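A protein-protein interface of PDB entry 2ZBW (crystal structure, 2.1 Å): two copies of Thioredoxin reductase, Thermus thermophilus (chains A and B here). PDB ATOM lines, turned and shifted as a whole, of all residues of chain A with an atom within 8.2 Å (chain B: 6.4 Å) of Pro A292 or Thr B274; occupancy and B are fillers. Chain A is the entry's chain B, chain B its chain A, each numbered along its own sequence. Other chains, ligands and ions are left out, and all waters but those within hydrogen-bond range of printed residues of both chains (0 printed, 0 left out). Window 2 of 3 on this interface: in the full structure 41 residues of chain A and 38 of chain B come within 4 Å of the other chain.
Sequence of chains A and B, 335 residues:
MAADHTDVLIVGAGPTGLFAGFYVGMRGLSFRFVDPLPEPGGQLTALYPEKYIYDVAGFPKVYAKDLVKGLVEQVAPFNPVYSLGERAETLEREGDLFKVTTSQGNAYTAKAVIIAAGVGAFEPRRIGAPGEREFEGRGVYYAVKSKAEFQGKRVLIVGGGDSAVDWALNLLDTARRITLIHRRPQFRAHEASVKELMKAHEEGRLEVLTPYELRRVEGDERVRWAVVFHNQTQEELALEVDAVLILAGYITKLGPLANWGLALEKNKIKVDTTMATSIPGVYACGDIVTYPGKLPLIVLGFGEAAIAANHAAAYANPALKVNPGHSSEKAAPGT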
ATOM      1  N   GLU A 265     -12.682   3.179  -1.580  1.00  0.00           N
ATOM      2  CA  GLU A 265     -14.089   3.135  -1.218  1.00  0.00           C
ATOM      3  C   GLU A 265     -14.837   2.939  -2.524  1.00  0.00           C
ATOM      4  O   GLU A 265     -14.908   3.846  -3.353  1.00  0.00           O
ATOM      5  CB  GLU A 265     -14.532   4.433  -0.540  1.00  0.00           C
ATOM      6  CG  GLU A 265     -15.876   4.303   0.160  1.00  0.00           C
ATOM      7  CD  GLU A 265     -16.199   5.485   1.058  1.00  0.00           C
ATOM      8  OE1 GLU A 265     -15.313   5.917   1.828  1.00  0.00           O
ATOM      9  OE2 GLU A 265     -17.347   5.974   1.005  1.00  0.00           O
ATOM     10  N   VAL A 271      -9.384  10.567  -0.743  1.00  0.00           N
ATOM     11  CA  VAL A 271      -8.418  11.657  -0.664  1.00  0.00           C
ATOM     12  C   VAL A 271      -8.937  12.761   0.245  1.00  0.00           C
ATOM     13  O   VAL A 271     -10.143  12.874   0.458  1.00  0.00           O
ATOM     14  CB  VAL A 271      -8.163  12.290  -2.053  1.00  0.00           C
ATOM     15  CG1 VAL A 271      -7.669  11.239  -3.035  1.00  0.00           C
ATOM     16  CG2 VAL A 271      -9.437  12.927  -2.571  1.00  0.00           C
ATOM     17  N   THR A 273      -8.763  17.070   1.106  1.00  0.00           N
ATOM     18  CA  THR A 273      -8.898  18.198   0.196  1.00  0.00           C
ATOM     19  C   THR A 273      -7.619  18.659  -0.507  1.00  0.00           C
ATOM     20  O   THR A 273      -7.682  19.478  -1.423  1.00  0.00           O
ATOM     21  CB  THR A 273      -9.580  19.394   0.892  1.00  0.00           C
ATOM     22  OG1 THR A 273      -8.766  19.866   1.974  1.00  0.00           O
ATOM     23  CG2 THR A 273     -10.943  18.962   1.436  1.00  0.00           C
ATOM     24  N   VAL A 289     -10.792   9.496  -7.890  1.00  0.00           N
ATOM     25  CA  VAL A 289     -10.909   9.847  -6.480  1.00  0.00           C
ATOM     26  C   VAL A 289     -12.343   9.919  -6.008  1.00  0.00           C
ATOM     27  O   VAL A 289     -13.278   9.977  -6.809  1.00  0.00           O
ATOM     28  CB  VAL A 289     -10.225  11.202  -6.151  1.00  0.00           C
ATOM     29  CG1 VAL A 289      -8.769  11.166  -6.578  1.00  0.00           C
ATOM     30  CG2 VAL A 289     -10.971  12.347  -6.824  1.00  0.00           C
ATOM     31  N   THR A 290     -12.509   9.892  -4.692  1.00  0.00           N
ATOM     32  CA  THR A 290     -13.830   9.993  -4.116  1.00  0.00           C
ATOM     33  C   THR A 290     -13.814  10.821  -2.848  1.00  0.00           C
ATOM     34  O   THR A 290     -12.855  10.795  -2.076  1.00  0.00           O
ATOM     35  CB  THR A 290     -14.432   8.627  -3.786  1.00  0.00           C
ATOM     36  OG1 THR A 290     -15.752   8.824  -3.264  1.00  0.00           O
ATOM     37  CG2 THR A 290     -13.586   7.893  -2.759  1.00  0.00           C
ATOM     38  N   TYR A 291     -14.885  11.581  -2.672  1.00  0.00           N
ATOM     39  CA  TYR A 291     -15.086  12.428  -1.513  1.00  0.00           C
ATOM     40  C   TYR A 291     -16.515  12.930  -1.668  1.00  0.00           C
ATOM     41  O   TYR A 291     -17.068  12.890  -2.771  1.00  0.00           O
ATOM     42  CB  TYR A 291     -14.053  13.576  -1.475  1.00  0.00           C
ATOM     43  CG  TYR A 291     -13.988  14.467  -2.700  1.00  0.00           C
ATOM     44  CD1 TYR A 291     -14.922  15.486  -2.895  1.00  0.00           C
ATOM     45  CD2 TYR A 291     -12.989  14.295  -3.661  1.00  0.00           C
ATOM     46  CE1 TYR A 291     -14.869  16.310  -4.009  1.00  0.00           C
ATOM     47  CE2 TYR A 291     -12.923  15.118  -4.785  1.00  0.00           C
ATOM     48  CZ  TYR A 291     -13.873  16.122  -4.951  1.00  0.00           C
ATOM     49  OH  TYR A 291     -13.849  16.918  -6.065  1.00  0.00           O
ATOM     50  N   PRO A 292     -17.152  13.369  -0.568  1.00  0.00           N
ATOM     51  CA  PRO A 292     -18.533  13.858  -0.658  1.00  0.00           C
ATOM     52  C   PRO A 292     -18.662  15.044  -1.607  1.00  0.00           C
ATOM     53  O   PRO A 292     -18.000  16.066  -1.431  1.00  0.00           O
ATOM     54  CB  PRO A 292     -18.864  14.231   0.789  1.00  0.00           C
ATOM     55  CG  PRO A 292     -17.989  13.303   1.594  1.00  0.00           C
ATOM     56  CD  PRO A 292     -16.684  13.362   0.828  1.00  0.00           C
ATOM     57  N   GLY A 293     -19.516  14.910  -2.613  1.00  0.00           N
ATOM     58  CA  GLY A 293     -19.695  15.997  -3.558  1.00  0.00           C
ATOM     59  C   GLY A 293     -18.900  15.811  -4.840  1.00  0.00           C
ATOM     60  O   GLY A 293     -19.011  16.610  -5.770  1.00  0.00           O
ATOM     61  N   LYS A 294     -18.083  14.765  -4.885  1.00  0.00           N
ATOM     62  CA  LYS A 294     -17.287  14.472  -6.072  1.00  0.00           C
ATOM     63  C   LYS A 294     -18.189  14.101  -7.254  1.00  0.00           C
ATOM     64  O   LYS A 294     -19.107  13.301  -7.111  1.00  0.00           O
ATOM     65  CB  LYS A 294     -16.327  13.312  -5.778  1.00  0.00           C
ATOM     66  CG  LYS A 294     -15.709  12.658  -7.014  1.00  0.00           C
ATOM     67  CD  LYS A 294     -14.840  13.630  -7.800  1.00  0.00           C
ATOM     68  CE  LYS A 294     -14.301  12.985  -9.070  1.00  0.00           C
ATOM     69  NZ  LYS A 294     -13.567  13.943  -9.940  1.00  0.00           N
ATOM     70  N   LEU A 295     -17.927  14.695  -8.412  1.00  0.00           N
ATOM     71  CA  LEU A 295     -18.689  14.416  -9.623  1.00  0.00           C
ATOM     72  C   LEU A 295     -17.706  14.001 -10.714  1.00  0.00           C
ATOM     73  O   LEU A 295     -16.635  14.608 -10.862  1.00  0.00           O
ATOM     74  CB  LEU A 295     -19.459  15.660 -10.080  1.00  0.00           C
ATOM     75  CG  LEU A 295     -20.457  16.289  -9.107  1.00  0.00           C
ATOM     76  CD1 LEU A 295     -21.109  17.503  -9.773  1.00  0.00           C
ATOM     77  CD2 LEU A 295     -21.504  15.259  -8.700  1.00  0.00           C
ATOM     78  N   LEU A 300     -14.106  19.395 -12.925  1.00  0.00           N
ATOM     79  CA  LEU A 300     -13.717  19.157 -11.547  1.00  0.00           C
ATOM     80  C   LEU A 300     -12.383  18.414 -11.552  1.00  0.00           C
ATOM     81  O   LEU A 300     -11.537  18.639 -10.687  1.00  0.00           O
ATOM     82  CB  LEU A 300     -14.788  18.330 -10.842  1.00  0.00           C
ATOM     83  CG  LEU A 300     -14.625  18.048  -9.355  1.00  0.00           C
ATOM     84  CD1 LEU A 300     -14.285  19.337  -8.610  1.00  0.00           C
ATOM     85  CD2 LEU A 300     -15.915  17.417  -8.829  1.00  0.00           C
ATOM     86  N   VAL B 271     -16.304  25.846   3.820  1.00  0.00           N
ATOM     87  CA  VAL B 271     -17.177  24.953   3.064  1.00  0.00           C
ATOM     88  C   VAL B 271     -16.756  23.493   3.188  1.00  0.00           C
ATOM     89  O   VAL B 271     -15.584  23.199   3.437  1.00  0.00           O
ATOM     90  CB  VAL B 271     -17.151  25.282   1.555  1.00  0.00           C
ATOM     91  CG1 VAL B 271     -17.819  26.611   1.285  1.00  0.00           C
ATOM     92  CG2 VAL B 271     -15.703  25.310   1.067  1.00  0.00           C
ATOM     93  N   ASP B 272     -17.708  22.575   3.024  1.00  0.00           N
ATOM     94  CA  ASP B 272     -17.352  21.167   3.052  1.00  0.00           C
ATOM     95  C   ASP B 272     -17.044  20.825   1.594  1.00  0.00           C
ATOM     96  O   ASP B 272     -17.085  21.711   0.727  1.00  0.00           O
ATOM     97  CB  ASP B 272     -18.484  20.282   3.623  1.00  0.00           C
ATOM     98  CG  ASP B 272     -19.796  20.417   2.873  1.00  0.00           C
ATOM     99  OD1 ASP B 272     -19.783  20.620   1.644  1.00  0.00           O
ATOM    100  OD2 ASP B 272     -20.857  20.296   3.522  1.00  0.00           O
ATOM    101  N   THR B 273     -16.741  19.562   1.316  1.00  0.00           N
ATOM    102  CA  THR B 273     -16.399  19.149  -0.041  1.00  0.00           C
ATOM    103  C   THR B 273     -17.525  19.246  -1.066  1.00  0.00           C
ATOM    104  O   THR B 273     -17.278  19.077  -2.260  1.00  0.00           O
ATOM    105  CB  THR B 273     -15.823  17.721  -0.058  1.00  0.00           C
ATOM    106  OG1 THR B 273     -16.802  16.801   0.423  1.00  0.00           O
ATOM    107  CG2 THR B 273     -14.581  17.644   0.837  1.00  0.00           C
ATOM    108  N   THR B 274     -18.759  19.496  -0.622  1.00  0.00           N
ATOM    109  CA  THR B 274     -19.865  19.649  -1.573  1.00  0.00           C
ATOM    110  C   THR B 274     -20.051  21.147  -1.840  1.00  0.00           C
ATOM    111  O   THR B 274     -20.942  21.550  -2.595  1.00  0.00           O
ATOM    112  CB  THR B 274     -21.201  19.071  -1.033  1.00  0.00           C
ATOM    113  OG1 THR B 274     -21.686  19.889   0.041  1.00  0.00           O
ATOM    114  CG2 THR B 274     -21.002  17.646  -0.529  1.00  0.00           C
ATOM    115  N   MET B 275     -19.200  21.958  -1.207  1.00  0.00           N
ATOM    116  CA  MET B 275     -19.217  23.425  -1.329  1.00  0.00           C
ATOM    117  C   MET B 275     -20.357  24.105  -0.578  1.00  0.00           C
ATOM    118  O   MET B 275     -20.657  25.283  -0.812  1.00  0.00           O
ATOM    119  CB  MET B 275     -19.260  23.859  -2.802  1.00  0.00           C
ATOM    120  CG  MET B 275     -17.959  23.668  -3.569  1.00  0.00           C
ATOM    121  SD  MET B 275     -16.494  24.699  -2.840  1.00  0.00           S
ATOM    122  CE  MET B 275     -15.426  23.246  -2.197  1.00  0.00           C
ATOM    123  N   ALA B 276     -20.993  23.371   0.327  1.00  0.00           N
ATOM    124  CA  ALA B 276     -22.085  23.937   1.106  1.00  0.00           C
ATOM    125  C   ALA B 276     -21.484  24.777   2.221  1.00  0.00           C
ATOM    126  O   ALA B 276     -20.453  24.403   2.786  1.00  0.00           O
ATOM    127  CB  ALA B 276     -22.943  22.823   1.698  1.00  0.00           C
ATOM    128  N   TYR B 283     -24.425  27.948  -0.962  1.00  0.00           N
ATOM    129  CA  TYR B 283     -23.195  27.303  -1.403  1.00  0.00           C
ATOM    130  C   TYR B 283     -22.245  28.400  -1.852  1.00  0.00           C
ATOM    131  O   TYR B 283     -22.675  29.525  -2.117  1.00  0.00           O
ATOM    132  CB  TYR B 283     -23.509  26.351  -2.560  1.00  0.00           C
ATOM    133  CG  TYR B 283     -24.500  25.278  -2.168  1.00  0.00           C
ATOM    134  CD1 TYR B 283     -24.067  24.039  -1.690  1.00  0.00           C
ATOM    135  CD2 TYR B 283     -25.873  25.529  -2.196  1.00  0.00           C
ATOM    136  CE1 TYR B 283     -24.977  23.079  -1.239  1.00  0.00           C
ATOM    137  CE2 TYR B 283     -26.790  24.581  -1.752  1.00  0.00           C
ATOM    138  CZ  TYR B 283     -26.337  23.362  -1.272  1.00  0.00           C
ATOM    139  OH  TYR B 283     -27.241  22.440  -0.808  1.00  0.00           O
ATOM    140  N   ALA B 284     -20.962  28.074  -1.935  1.00  0.00           N
ATOM    141  CA  ALA B 284     -19.954  29.046  -2.351  1.00  0.00           C
ATOM    142  C   ALA B 284     -18.861  28.369  -3.174  1.00  0.00           C
ATOM    143  O   ALA B 284     -18.722  27.158  -3.140  1.00  0.00           O
ATOM    144  CB  ALA B 284     -19.347  29.728  -1.128  1.00  0.00           C
ATOM    145  N   GLU B 304     -14.835  24.059  -8.293  1.00  0.00           N
ATOM    146  CA  GLU B 304     -15.640  24.360  -7.121  1.00  0.00           C
ATOM    147  C   GLU B 304     -17.013  24.873  -7.546  1.00  0.00           C
ATOM    148  O   GLU B 304     -18.015  24.592  -6.887  1.00  0.00           O
ATOM    149  CB  GLU B 304     -14.930  25.406  -6.266  1.00  0.00           C
ATOM    150  CG  GLU B 304     -13.618  24.917  -5.642  1.00  0.00           C
ATOM    151  CD  GLU B 304     -12.774  26.063  -5.127  1.00  0.00           C
ATOM    152  OE1 GLU B 304     -11.765  25.810  -4.431  1.00  0.00           O
ATOM    153  OE2 GLU B 304     -13.125  27.221  -5.428  1.00  0.00           O
ATOM    154  N   ILE B 307     -19.265  22.035  -8.593  1.00  0.00           N
ATOM    155  CA  ILE B 307     -19.760  21.331  -7.425  1.00  0.00           C
ATOM    156  C   ILE B 307     -20.871  22.122  -6.732  1.00  0.00           C
ATOM    157  O   ILE B 307     -21.881  21.545  -6.322  1.00  0.00           O
ATOM    158  CB  ILE B 307     -18.617  21.034  -6.419  1.00  0.00           C
ATOM    159  CG1 ILE B 307     -17.640  20.023  -7.038  1.00  0.00           C
ATOM    160  CG2 ILE B 307     -19.185  20.478  -5.116  1.00  0.00           C
ATOM    161  CD1 ILE B 307     -16.453  19.653  -6.136  1.00  0.00           C
ATOM    162  N   ALA B 308     -20.697  23.438  -6.621  1.00  0.00           N
ATOM    163  CA  ALA B 308     -21.700  24.281  -5.969  1.00  0.00           C
ATOM    164  C   ALA B 308     -22.958  24.433  -6.812  1.00  0.00           C
ATOM    165  O   ALA B 308     -24.065  24.402  -6.290  1.00  0.00           O
ATOM    166  CB  ALA B 308     -21.114  25.664  -5.660  1.00  0.00           C
ATOM    167  N   HIS B 311     -25.006  21.062  -6.719  1.00  0.00           N
ATOM    168  CA  HIS B 311     -25.584  20.797  -5.410  1.00  0.00           C
ATOM    169  C   HIS B 311     -26.642  21.859  -5.103  1.00  0.00           C
ATOM    170  O   HIS B 311     -27.638  21.589  -4.432  1.00  0.00           O
ATOM    171  CB  HIS B 311     -24.510  20.824  -4.318  1.00  0.00           C
ATOM    172  CG  HIS B 311     -23.683  19.578  -4.252  1.00  0.00           C
ATOM    173  ND1 HIS B 311     -22.624  19.340  -5.099  1.00  0.00           N
ATOM    174  CD2 HIS B 311     -23.791  18.480  -3.465  1.00  0.00           C
ATOM    175  CE1 HIS B 311     -22.113  18.149  -4.837  1.00  0.00           C
ATOM    176  NE2 HIS B 311     -22.804  17.607  -3.851  1.00  0.00           N
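The backbone carbonyl oxygen of Pro A292 sits close to the side-chain hydroxyl of Thr B273 (2.3 Å).
Thr B273 touches its own counterpart, Thr A273. 2 positions are printed for both chains. Of the 9 pairs that touch across the chains among the printed residues, 1 has its exchanged pair printed and touching as well.
A ring nitrogen (ND1) of His B311 sits at hydrogen-bond distance from the backbone carbonyl oxygen (O) of Ile B307. OD1 of Asp B272 lies within hydrogen-bond range of OG1 of Thr B274, 2.6 Å away.
Of the printed residues of chain B, Tyr A291 touches Thr B273 (3.7 Å) and Ile B307 (3.8 Å). Of chain B, only Thr B273 and Thr B274 come within 4 Å of Pro A292. Of the printed residues of chain B, Gly A293 touches Thr B274, Ile B307 and His B311. Of the printed residues of chain A, Thr B273 touches Thr A273, Tyr A291 and Pro A292. Of chain A, only Pro A292 (3.5 Å) and Gly A293 (3.7 Å) come within 4 Å of Thr B274. Met B275 touches none of the printed residues of chain A. Of the printed residues of chain A, Ile B307 touches Tyr A291 (3.8 Å), Gly A293 (3.9 Å) and Leu A300 (3.3 Å). Of the printed residues of chain A, His B311 touches Gly A293 (3.5 Å). The nearest printed residue of chain A that does not touch Thr B274 is Lys A294 (6.0 Å). The nearest printed residue of chain A that does not touch Ile B307 is Leu A295 (4.7 Å).
Among the printed residues, pairs that only touch across the chains: Thr A273 with Thr B273 (3.9 Å), Tyr A291 with Thr B273 (3.7 Å), Tyr A291 with Ile B307 (3.8 Å), Pro A292 with Thr B274 (3.5 Å), Gly A293 with Thr B274 (3.7 Å), Gly A293 with Ile B307 (3.9 Å), Gly A293 with His B311 (3.5 Å) and Leu A300 with Ile B307 (3.3 Å).
Of the 11 printed residues of chain A, 5 touch a printed residue of chain B. Hydrophobic or aromatic side chains of chain A that line the printed part of chain B: Tyr A291, Pro A292 and Leu A300. Among the printed residues, 9 pairs touch across the chains.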
